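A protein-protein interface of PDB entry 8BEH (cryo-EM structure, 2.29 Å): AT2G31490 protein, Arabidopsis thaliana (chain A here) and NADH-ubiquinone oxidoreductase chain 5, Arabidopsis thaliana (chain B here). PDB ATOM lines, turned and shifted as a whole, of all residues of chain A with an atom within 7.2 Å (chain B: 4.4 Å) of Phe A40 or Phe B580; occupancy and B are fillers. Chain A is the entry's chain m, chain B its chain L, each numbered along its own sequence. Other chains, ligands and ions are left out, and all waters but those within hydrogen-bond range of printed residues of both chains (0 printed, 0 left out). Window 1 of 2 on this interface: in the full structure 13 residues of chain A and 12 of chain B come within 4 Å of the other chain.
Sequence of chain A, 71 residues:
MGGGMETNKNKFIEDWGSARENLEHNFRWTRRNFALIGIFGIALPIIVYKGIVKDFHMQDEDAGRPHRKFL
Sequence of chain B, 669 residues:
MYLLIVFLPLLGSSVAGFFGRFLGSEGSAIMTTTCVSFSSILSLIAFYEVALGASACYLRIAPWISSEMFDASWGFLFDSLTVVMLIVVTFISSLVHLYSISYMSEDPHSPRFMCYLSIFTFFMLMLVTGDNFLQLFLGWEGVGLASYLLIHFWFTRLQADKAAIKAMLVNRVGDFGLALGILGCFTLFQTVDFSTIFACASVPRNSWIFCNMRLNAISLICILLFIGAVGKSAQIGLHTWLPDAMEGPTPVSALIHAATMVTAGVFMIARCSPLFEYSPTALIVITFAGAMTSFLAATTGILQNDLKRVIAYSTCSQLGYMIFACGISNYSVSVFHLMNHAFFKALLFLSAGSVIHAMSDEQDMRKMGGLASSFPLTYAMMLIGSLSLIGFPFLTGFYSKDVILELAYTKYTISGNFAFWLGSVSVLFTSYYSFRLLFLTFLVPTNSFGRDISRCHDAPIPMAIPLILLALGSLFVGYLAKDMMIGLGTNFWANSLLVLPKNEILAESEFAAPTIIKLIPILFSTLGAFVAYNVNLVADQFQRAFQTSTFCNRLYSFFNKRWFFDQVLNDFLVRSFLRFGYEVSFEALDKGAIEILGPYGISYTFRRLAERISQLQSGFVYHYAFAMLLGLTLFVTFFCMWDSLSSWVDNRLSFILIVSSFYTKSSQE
N of Ser B585 sits at hydrogen-bond distance from O of Phe B580, 3.3 Å away.
Leu A36 touches Val B584 (CD2 to CG2, 3.99 Å).
Phe A40 touches Phe B580 (CD1 to CE2, 3.5 Å).
CB of Phe A40 touches CG1 of Val B584, 3.6 Å away.
Of chain B, only Phe B580 (3.5 Å) and Val B584 (3.6 Å) come within 4 Å of Phe A40.
Phe B580 touches one residue of chain A.
Of the printed residues of chain A, Val B584 touches Leu A36 and Phe A40.
Of the printed residues of chain B, Leu A36 touches Val B584 (3.99 Å).
The nearest printed residue of chain B that does not touch Phe A40 is Ser B585 (6.6 Å).
Of the 12 printed residues of chain A, 2 touch a printed residue of chain B.
Printed residues of chain A that touch a printed residue of chain B: Leu A36 and Phe A40.
Of the 10 printed residues of chain B, 2 touch a printed residue of chain A.
Hydrophobic or aromatic side chains of chain B that line the printed part of chain A: Phe B580 and Val B584.
Among the printed residues, no Asp or Glu carboxylate lies within 4 Å of a Lys or Arg side-chain nitrogen of the other chain.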
ATOM      1  N   PHE A  34      -4.841 -34.171 -10.796  1.00  0.00           N
ATOM      2  CA  PHE A  34      -5.730 -34.444  -9.675  1.00  0.00           C
ATOM      3  C   PHE A  34      -5.411 -33.530  -8.500  1.00  0.00           C
ATOM      4  O   PHE A  34      -6.312 -32.947  -7.891  1.00  0.00           O
ATOM      5  CB  PHE A  34      -5.624 -35.912  -9.258  1.00  0.00           C
ATOM      6  CG  PHE A  34      -6.723 -36.774  -9.799  1.00  0.00           C
ATOM      7  CD1 PHE A  34      -6.429 -37.925 -10.512  1.00  0.00           C
ATOM      8  CD2 PHE A  34      -8.048 -36.423  -9.624  1.00  0.00           C
ATOM      9  CE1 PHE A  34      -7.435 -38.717 -11.023  1.00  0.00           C
ATOM     10  CE2 PHE A  34      -9.062 -37.210 -10.136  1.00  0.00           C
ATOM     11  CZ  PHE A  34      -8.754 -38.358 -10.837  1.00  0.00           C
ATOM     12  N   ALA A  35      -4.123 -33.375  -8.187  1.00  0.00           N
ATOM     13  CA  ALA A  35      -3.727 -32.494  -7.095  1.00  0.00           C
ATOM     14  C   ALA A  35      -4.094 -31.044  -7.395  1.00  0.00           C
ATOM     15  O   ALA A  35      -4.647 -30.346  -6.540  1.00  0.00           O
ATOM     16  CB  ALA A  35      -2.228 -32.627  -6.825  1.00  0.00           C
ATOM     17  N   LEU A  36      -3.854 -30.609  -8.641  1.00  0.00           N
ATOM     18  CA  LEU A  36      -4.084 -29.181  -8.973  1.00  0.00           C
ATOM     19  C   LEU A  36      -5.589 -28.858  -8.942  1.00  0.00           C
ATOM     20  O   LEU A  36      -5.940 -27.821  -8.440  1.00  0.00           O
ATOM     21  CB  LEU A  36      -3.371 -28.758 -10.268  1.00  0.00           C
ATOM     22  CG  LEU A  36      -1.853 -28.626 -10.253  1.00  0.00           C
ATOM     23  CD1 LEU A  36      -1.365 -28.229 -11.634  1.00  0.00           C
ATOM     24  CD2 LEU A  36      -1.392 -27.631  -9.214  1.00  0.00           C
ATOM     25  N   ILE A  37      -6.405 -29.788  -9.370  1.00  0.00           N
ATOM     26  CA  ILE A  37      -7.846 -29.567  -9.337  1.00  0.00           C
ATOM     27  C   ILE A  37      -8.373 -29.671  -7.912  1.00  0.00           C
ATOM     28  O   ILE A  37      -9.264 -28.916  -7.511  1.00  0.00           O
ATOM     29  CB  ILE A  37      -8.549 -30.544 -10.294  1.00  0.00           C
ATOM     30  CG1 ILE A  37      -8.116 -30.252 -11.732  1.00  0.00           C
ATOM     31  CG2 ILE A  37     -10.060 -30.453 -10.152  1.00  0.00           C
ATOM     32  CD1 ILE A  37      -8.727 -31.173 -12.760  1.00  0.00           C
ATOM     33  N   GLY A  38      -7.840 -30.607  -7.127  1.00  0.00           N
ATOM     34  CA  GLY A  38      -8.247 -30.708  -5.739  1.00  0.00           C
ATOM     35  C   GLY A  38      -7.874 -29.493  -4.916  1.00  0.00           C
ATOM     36  O   GLY A  38      -8.643 -29.067  -4.051  1.00  0.00           O
ATOM     37  N   ILE A  39      -6.703 -28.915  -5.173  1.00  0.00           N
ATOM     38  CA  ILE A  39      -6.236 -27.792  -4.371  1.00  0.00           C
ATOM     39  C   ILE A  39      -6.920 -26.500  -4.796  1.00  0.00           C
ATOM     40  O   ILE A  39      -7.504 -25.790  -3.973  1.00  0.00           O
ATOM     41  CB  ILE A  39      -4.705 -27.674  -4.461  1.00  0.00           C
ATOM     42  CG1 ILE A  39      -4.038 -28.830  -3.714  1.00  0.00           C
ATOM     43  CG2 ILE A  39      -4.237 -26.328  -3.913  1.00  0.00           C
ATOM     44  CD1 ILE A  39      -2.683 -29.201  -4.254  1.00  0.00           C
ATOM     45  N   PHE A  40      -6.914 -26.237  -6.099  1.00  0.00           N
ATOM     46  CA  PHE A  40      -7.353 -24.925  -6.625  1.00  0.00           C
ATOM     47  C   PHE A  40      -8.806 -24.919  -7.069  1.00  0.00           C
ATOM     48  O   PHE A  40      -9.393 -23.917  -7.106  1.00  0.00           O
ATOM     49  CB  PHE A  40      -6.349 -24.474  -7.673  1.00  0.00           C
ATOM     50  CG  PHE A  40      -4.994 -24.182  -7.087  1.00  0.00           C
ATOM     51  CD1 PHE A  40      -4.826 -23.122  -6.209  1.00  0.00           C
ATOM     52  CD2 PHE A  40      -3.895 -24.964  -7.396  1.00  0.00           C
ATOM     53  CE1 PHE A  40      -3.583 -22.845  -5.662  1.00  0.00           C
ATOM     54  CE2 PHE A  40      -2.653 -24.688  -6.847  1.00  0.00           C
ATOM     55  CZ  PHE A  40      -2.498 -23.626  -5.984  1.00  0.00           C
ATOM     56  N   GLY A  41      -9.331 -26.086  -7.325  1.00  0.00           N
ATOM     57  CA  GLY A  41     -10.692 -26.148  -7.813  1.00  0.00           C
ATOM     58  C   GLY A  41     -11.705 -26.402  -6.720  1.00  0.00           C
ATOM     59  O   GLY A  41     -12.888 -26.100  -6.888  1.00  0.00           O
ATOM     60  N   ILE A  42     -11.257 -26.950  -5.593  1.00  0.00           N
ATOM     61  CA  ILE A  42     -12.162 -27.305  -4.506  1.00  0.00           C
ATOM     62  C   ILE A  42     -11.716 -26.655  -3.202  1.00  0.00           C
ATOM     63  O   ILE A  42     -12.472 -25.889  -2.595  1.00  0.00           O
ATOM     64  CB  ILE A  42     -12.270 -28.835  -4.354  1.00  0.00           C
ATOM     65  CG1 ILE A  42     -13.114 -29.425  -5.485  1.00  0.00           C
ATOM     66  CG2 ILE A  42     -12.870 -29.211  -3.012  1.00  0.00           C
ATOM     67  CD1 ILE A  42     -12.305 -29.962  -6.616  1.00  0.00           C
ATOM     68  N   ALA A  43     -10.485 -26.945  -2.770  1.00  0.00           N
ATOM     69  CA  ALA A  43     -10.049 -26.541  -1.434  1.00  0.00           C
ATOM     70  C   ALA A  43      -9.994 -25.023  -1.288  1.00  0.00           C
ATOM     71  O   ALA A  43     -10.578 -24.461  -0.355  1.00  0.00           O
ATOM     72  CB  ALA A  43      -8.690 -27.162  -1.113  1.00  0.00           C
ATOM     73  N   LEU A  44      -9.303 -24.342  -2.203  1.00  0.00           N
ATOM     74  CA  LEU A  44      -9.156 -22.891  -2.090  1.00  0.00           C
ATOM     75  C   LEU A  44     -10.490 -22.150  -2.121  1.00  0.00           C
ATOM     76  O   LEU A  44     -10.686 -21.251  -1.286  1.00  0.00           O
ATOM     77  CB  LEU A  44      -8.203 -22.377  -3.175  1.00  0.00           C
ATOM     78  CG  LEU A  44      -7.734 -20.928  -3.032  1.00  0.00           C
ATOM     79  CD1 LEU A  44      -7.415 -20.596  -1.578  1.00  0.00           C
ATOM     80  CD2 LEU A  44      -6.539 -20.641  -3.926  1.00  0.00           C
ATOM     81  N   PRO A  45     -11.427 -22.445  -3.032  1.00  0.00           N
ATOM     82  CA  PRO A  45     -12.751 -21.806  -2.927  1.00  0.00           C
ATOM     83  C   PRO A  45     -13.446 -22.064  -1.601  1.00  0.00           C
ATOM     84  O   PRO A  45     -14.094 -21.159  -1.068  1.00  0.00           O
ATOM     85  CB  PRO A  45     -13.521 -22.417  -4.104  1.00  0.00           C
ATOM     86  CG  PRO A  45     -12.474 -22.795  -5.070  1.00  0.00           C
ATOM     87  CD  PRO A  45     -11.319 -23.255  -4.258  1.00  0.00           C
ATOM     88  N   SER B 576       5.773 -17.787  -9.983  1.00  0.00           N
ATOM     89  CA  SER B 576       4.653 -18.538  -9.425  1.00  0.00           C
ATOM     90  C   SER B 576       3.330 -18.095 -10.037  1.00  0.00           C
ATOM     91  O   SER B 576       2.544 -18.923 -10.509  1.00  0.00           O
ATOM     92  CB  SER B 576       4.619 -18.383  -7.904  1.00  0.00           C
ATOM     93  OG  SER B 576       5.352 -19.408  -7.269  1.00  0.00           O
ATOM     94  N   PHE B 577       3.066 -16.785 -10.037  1.00  0.00           N
ATOM     95  CA  PHE B 577       1.826 -16.293 -10.638  1.00  0.00           C
ATOM     96  C   PHE B 577       1.762 -16.574 -12.138  1.00  0.00           C
ATOM     97  O   PHE B 577       0.714 -16.991 -12.654  1.00  0.00           O
ATOM     98  CB  PHE B 577       1.635 -14.804 -10.346  1.00  0.00           C
ATOM     99  CG  PHE B 577       1.198 -14.518  -8.942  1.00  0.00           C
ATOM    100  CD1 PHE B 577       2.108 -14.339  -7.923  1.00  0.00           C
ATOM    101  CD2 PHE B 577      -0.149 -14.424  -8.644  1.00  0.00           C
ATOM    102  CE1 PHE B 577       1.679 -14.088  -6.634  1.00  0.00           C
ATOM    103  CE2 PHE B 577      -0.575 -14.165  -7.362  1.00  0.00           C
ATOM    104  CZ  PHE B 577       0.346 -13.996  -6.356  1.00  0.00           C
ATOM    105  N   LEU B 578       2.869 -16.364 -12.852  1.00  0.00           N
ATOM    106  CA  LEU B 578       2.874 -16.610 -14.289  1.00  0.00           C
ATOM    107  C   LEU B 578       2.583 -18.074 -14.599  1.00  0.00           C
ATOM    108  O   LEU B 578       1.823 -18.382 -15.523  1.00  0.00           O
ATOM    109  CB  LEU B 578       4.218 -16.193 -14.876  1.00  0.00           C
ATOM    110  CG  LEU B 578       4.367 -14.711 -15.213  1.00  0.00           C
ATOM    111  CD1 LEU B 578       5.746 -14.452 -15.793  1.00  0.00           C
ATOM    112  CD2 LEU B 578       3.280 -14.264 -16.177  1.00  0.00           C
ATOM    113  N   ARG B 579       3.131 -18.991 -13.816  1.00  0.00           N
ATOM    114  CA  ARG B 579       2.918 -20.444 -14.022  1.00  0.00           C
ATOM    115  C   ARG B 579       1.485 -20.848 -13.689  1.00  0.00           C
ATOM    116  O   ARG B 579       0.973 -21.651 -14.467  1.00  0.00           O
ATOM    117  CB  ARG B 579       3.953 -21.315 -13.304  1.00  0.00           C
ATOM    118  CG  ARG B 579       5.337 -21.230 -13.920  1.00  0.00           C
ATOM    119  CD  ARG B 579       6.195 -22.164 -13.114  1.00  0.00           C
ATOM    120  NE  ARG B 579       5.626 -23.486 -13.260  1.00  0.00           N
ATOM    121  CZ  ARG B 579       5.946 -24.520 -12.508  1.00  0.00           C
ATOM    122  NH1 ARG B 579       6.811 -24.375 -11.526  1.00  0.00           N
ATOM    123  NH2 ARG B 579       5.380 -25.687 -12.726  1.00  0.00           N
ATOM    124  N   PHE B 580       0.893 -20.275 -12.655  1.00  0.00           N
ATOM    125  CA  PHE B 580      -0.512 -20.504 -12.294  1.00  0.00           C
ATOM    126  C   PHE B 580      -1.398 -20.099 -13.454  1.00  0.00           C
ATOM    127  O   PHE B 580      -2.310 -20.851 -13.735  1.00  0.00           O
ATOM    128  CB  PHE B 580      -0.949 -19.740 -11.041  1.00  0.00           C
ATOM    129  CG  PHE B 580      -2.320 -20.004 -10.488  1.00  0.00           C
ATOM    130  CD1 PHE B 580      -3.423 -19.328 -10.977  1.00  0.00           C
ATOM    131  CD2 PHE B 580      -2.494 -20.872  -9.422  1.00  0.00           C
ATOM    132  CE1 PHE B 580      -4.678 -19.553 -10.438  1.00  0.00           C
ATOM    133  CE2 PHE B 580      -3.751 -21.096  -8.891  1.00  0.00           C
ATOM    134  CZ  PHE B 580      -4.840 -20.431  -9.395  1.00  0.00           C
ATOM    135  N   GLY B 581      -1.084 -18.941 -14.013  1.00  0.00           N
ATOM    136  CA  GLY B 581      -1.967 -18.470 -15.062  1.00  0.00           C
ATOM    137  C   GLY B 581      -2.149 -19.457 -16.199  1.00  0.00           C
ATOM    138  O   GLY B 581      -3.229 -19.537 -16.786  1.00  0.00           O
ATOM    139  N   TYR B 582      -1.109 -20.235 -16.552  1.00  0.00           N
ATOM    140  CA  TYR B 582      -1.151 -21.239 -17.665  1.00  0.00           C
ATOM    141  C   TYR B 582      -1.488 -22.658 -17.163  1.00  0.00           C
ATOM    142  O   TYR B 582      -2.504 -23.151 -17.552  1.00  0.00           O
ATOM    143  CB  TYR B 582       0.148 -21.223 -18.502  1.00  0.00           C
ATOM    144  CG  TYR B 582       0.119 -22.177 -19.667  1.00  0.00           C
ATOM    145  CD1 TYR B 582      -0.470 -21.803 -20.861  1.00  0.00           C
ATOM    146  CD2 TYR B 582       0.609 -23.468 -19.563  1.00  0.00           C
ATOM    147  CE1 TYR B 582      -0.539 -22.670 -21.931  1.00  0.00           C
ATOM    148  CE2 TYR B 582       0.546 -24.353 -20.624  1.00  0.00           C
ATOM    149  CZ  TYR B 582      -0.023 -23.946 -21.817  1.00  0.00           C
ATOM    150  OH  TYR B 582      -0.107 -24.778 -22.885  1.00  0.00           O
ATOM    151  N   GLU B 583      -0.720 -23.205 -16.247  1.00  0.00           N
ATOM    152  CA  GLU B 583      -0.864 -24.578 -15.689  1.00  0.00           C
ATOM    153  C   GLU B 583      -2.083 -24.861 -14.785  1.00  0.00           C
ATOM    154  O   GLU B 583      -2.476 -25.983 -14.773  1.00  0.00           O
ATOM    155  CB  GLU B 583       0.440 -24.931 -15.003  1.00  0.00           C
ATOM    156  CG  GLU B 583       1.608 -24.982 -15.964  1.00  0.00           C
ATOM    157  CD  GLU B 583       2.933 -24.684 -15.298  1.00  0.00           C
ATOM    158  OE1 GLU B 583       3.292 -25.424 -14.379  1.00  0.00           O
ATOM    159  OE2 GLU B 583       3.588 -23.700 -15.690  1.00  0.00           O
ATOM    160  N   VAL B 584      -2.730 -23.882 -14.159  1.00  0.00           N
ATOM    161  CA  VAL B 584      -3.836 -24.190 -13.230  1.00  0.00           C
ATOM    162  C   VAL B 584      -5.138 -23.620 -13.768  1.00  0.00           C
ATOM    163  O   VAL B 584      -6.010 -24.400 -14.090  1.00  0.00           O
ATOM    164  CB  VAL B 584      -3.504 -23.742 -11.767  1.00  0.00           C
ATOM    165  CG1 VAL B 584      -4.651 -23.963 -10.805  1.00  0.00           C
ATOM    166  CG2 VAL B 584      -2.194 -24.302 -11.258  1.00  0.00           C
ATOM    167  N   SER B 585      -5.239 -22.321 -13.802  1.00  0.00           N
ATOM    168  CA  SER B 585      -6.414 -21.567 -14.226  1.00  0.00           C
ATOM    169  C   SER B 585      -6.851 -21.904 -15.662  1.00  0.00           C
ATOM    170  O   SER B 585      -8.005 -22.069 -15.844  1.00  0.00           O
ATOM    171  CB  SER B 585      -6.142 -20.072 -13.978  1.00  0.00           C
ATOM    172  OG  SER B 585      -5.133 -19.552 -14.800  1.00  0.00           O
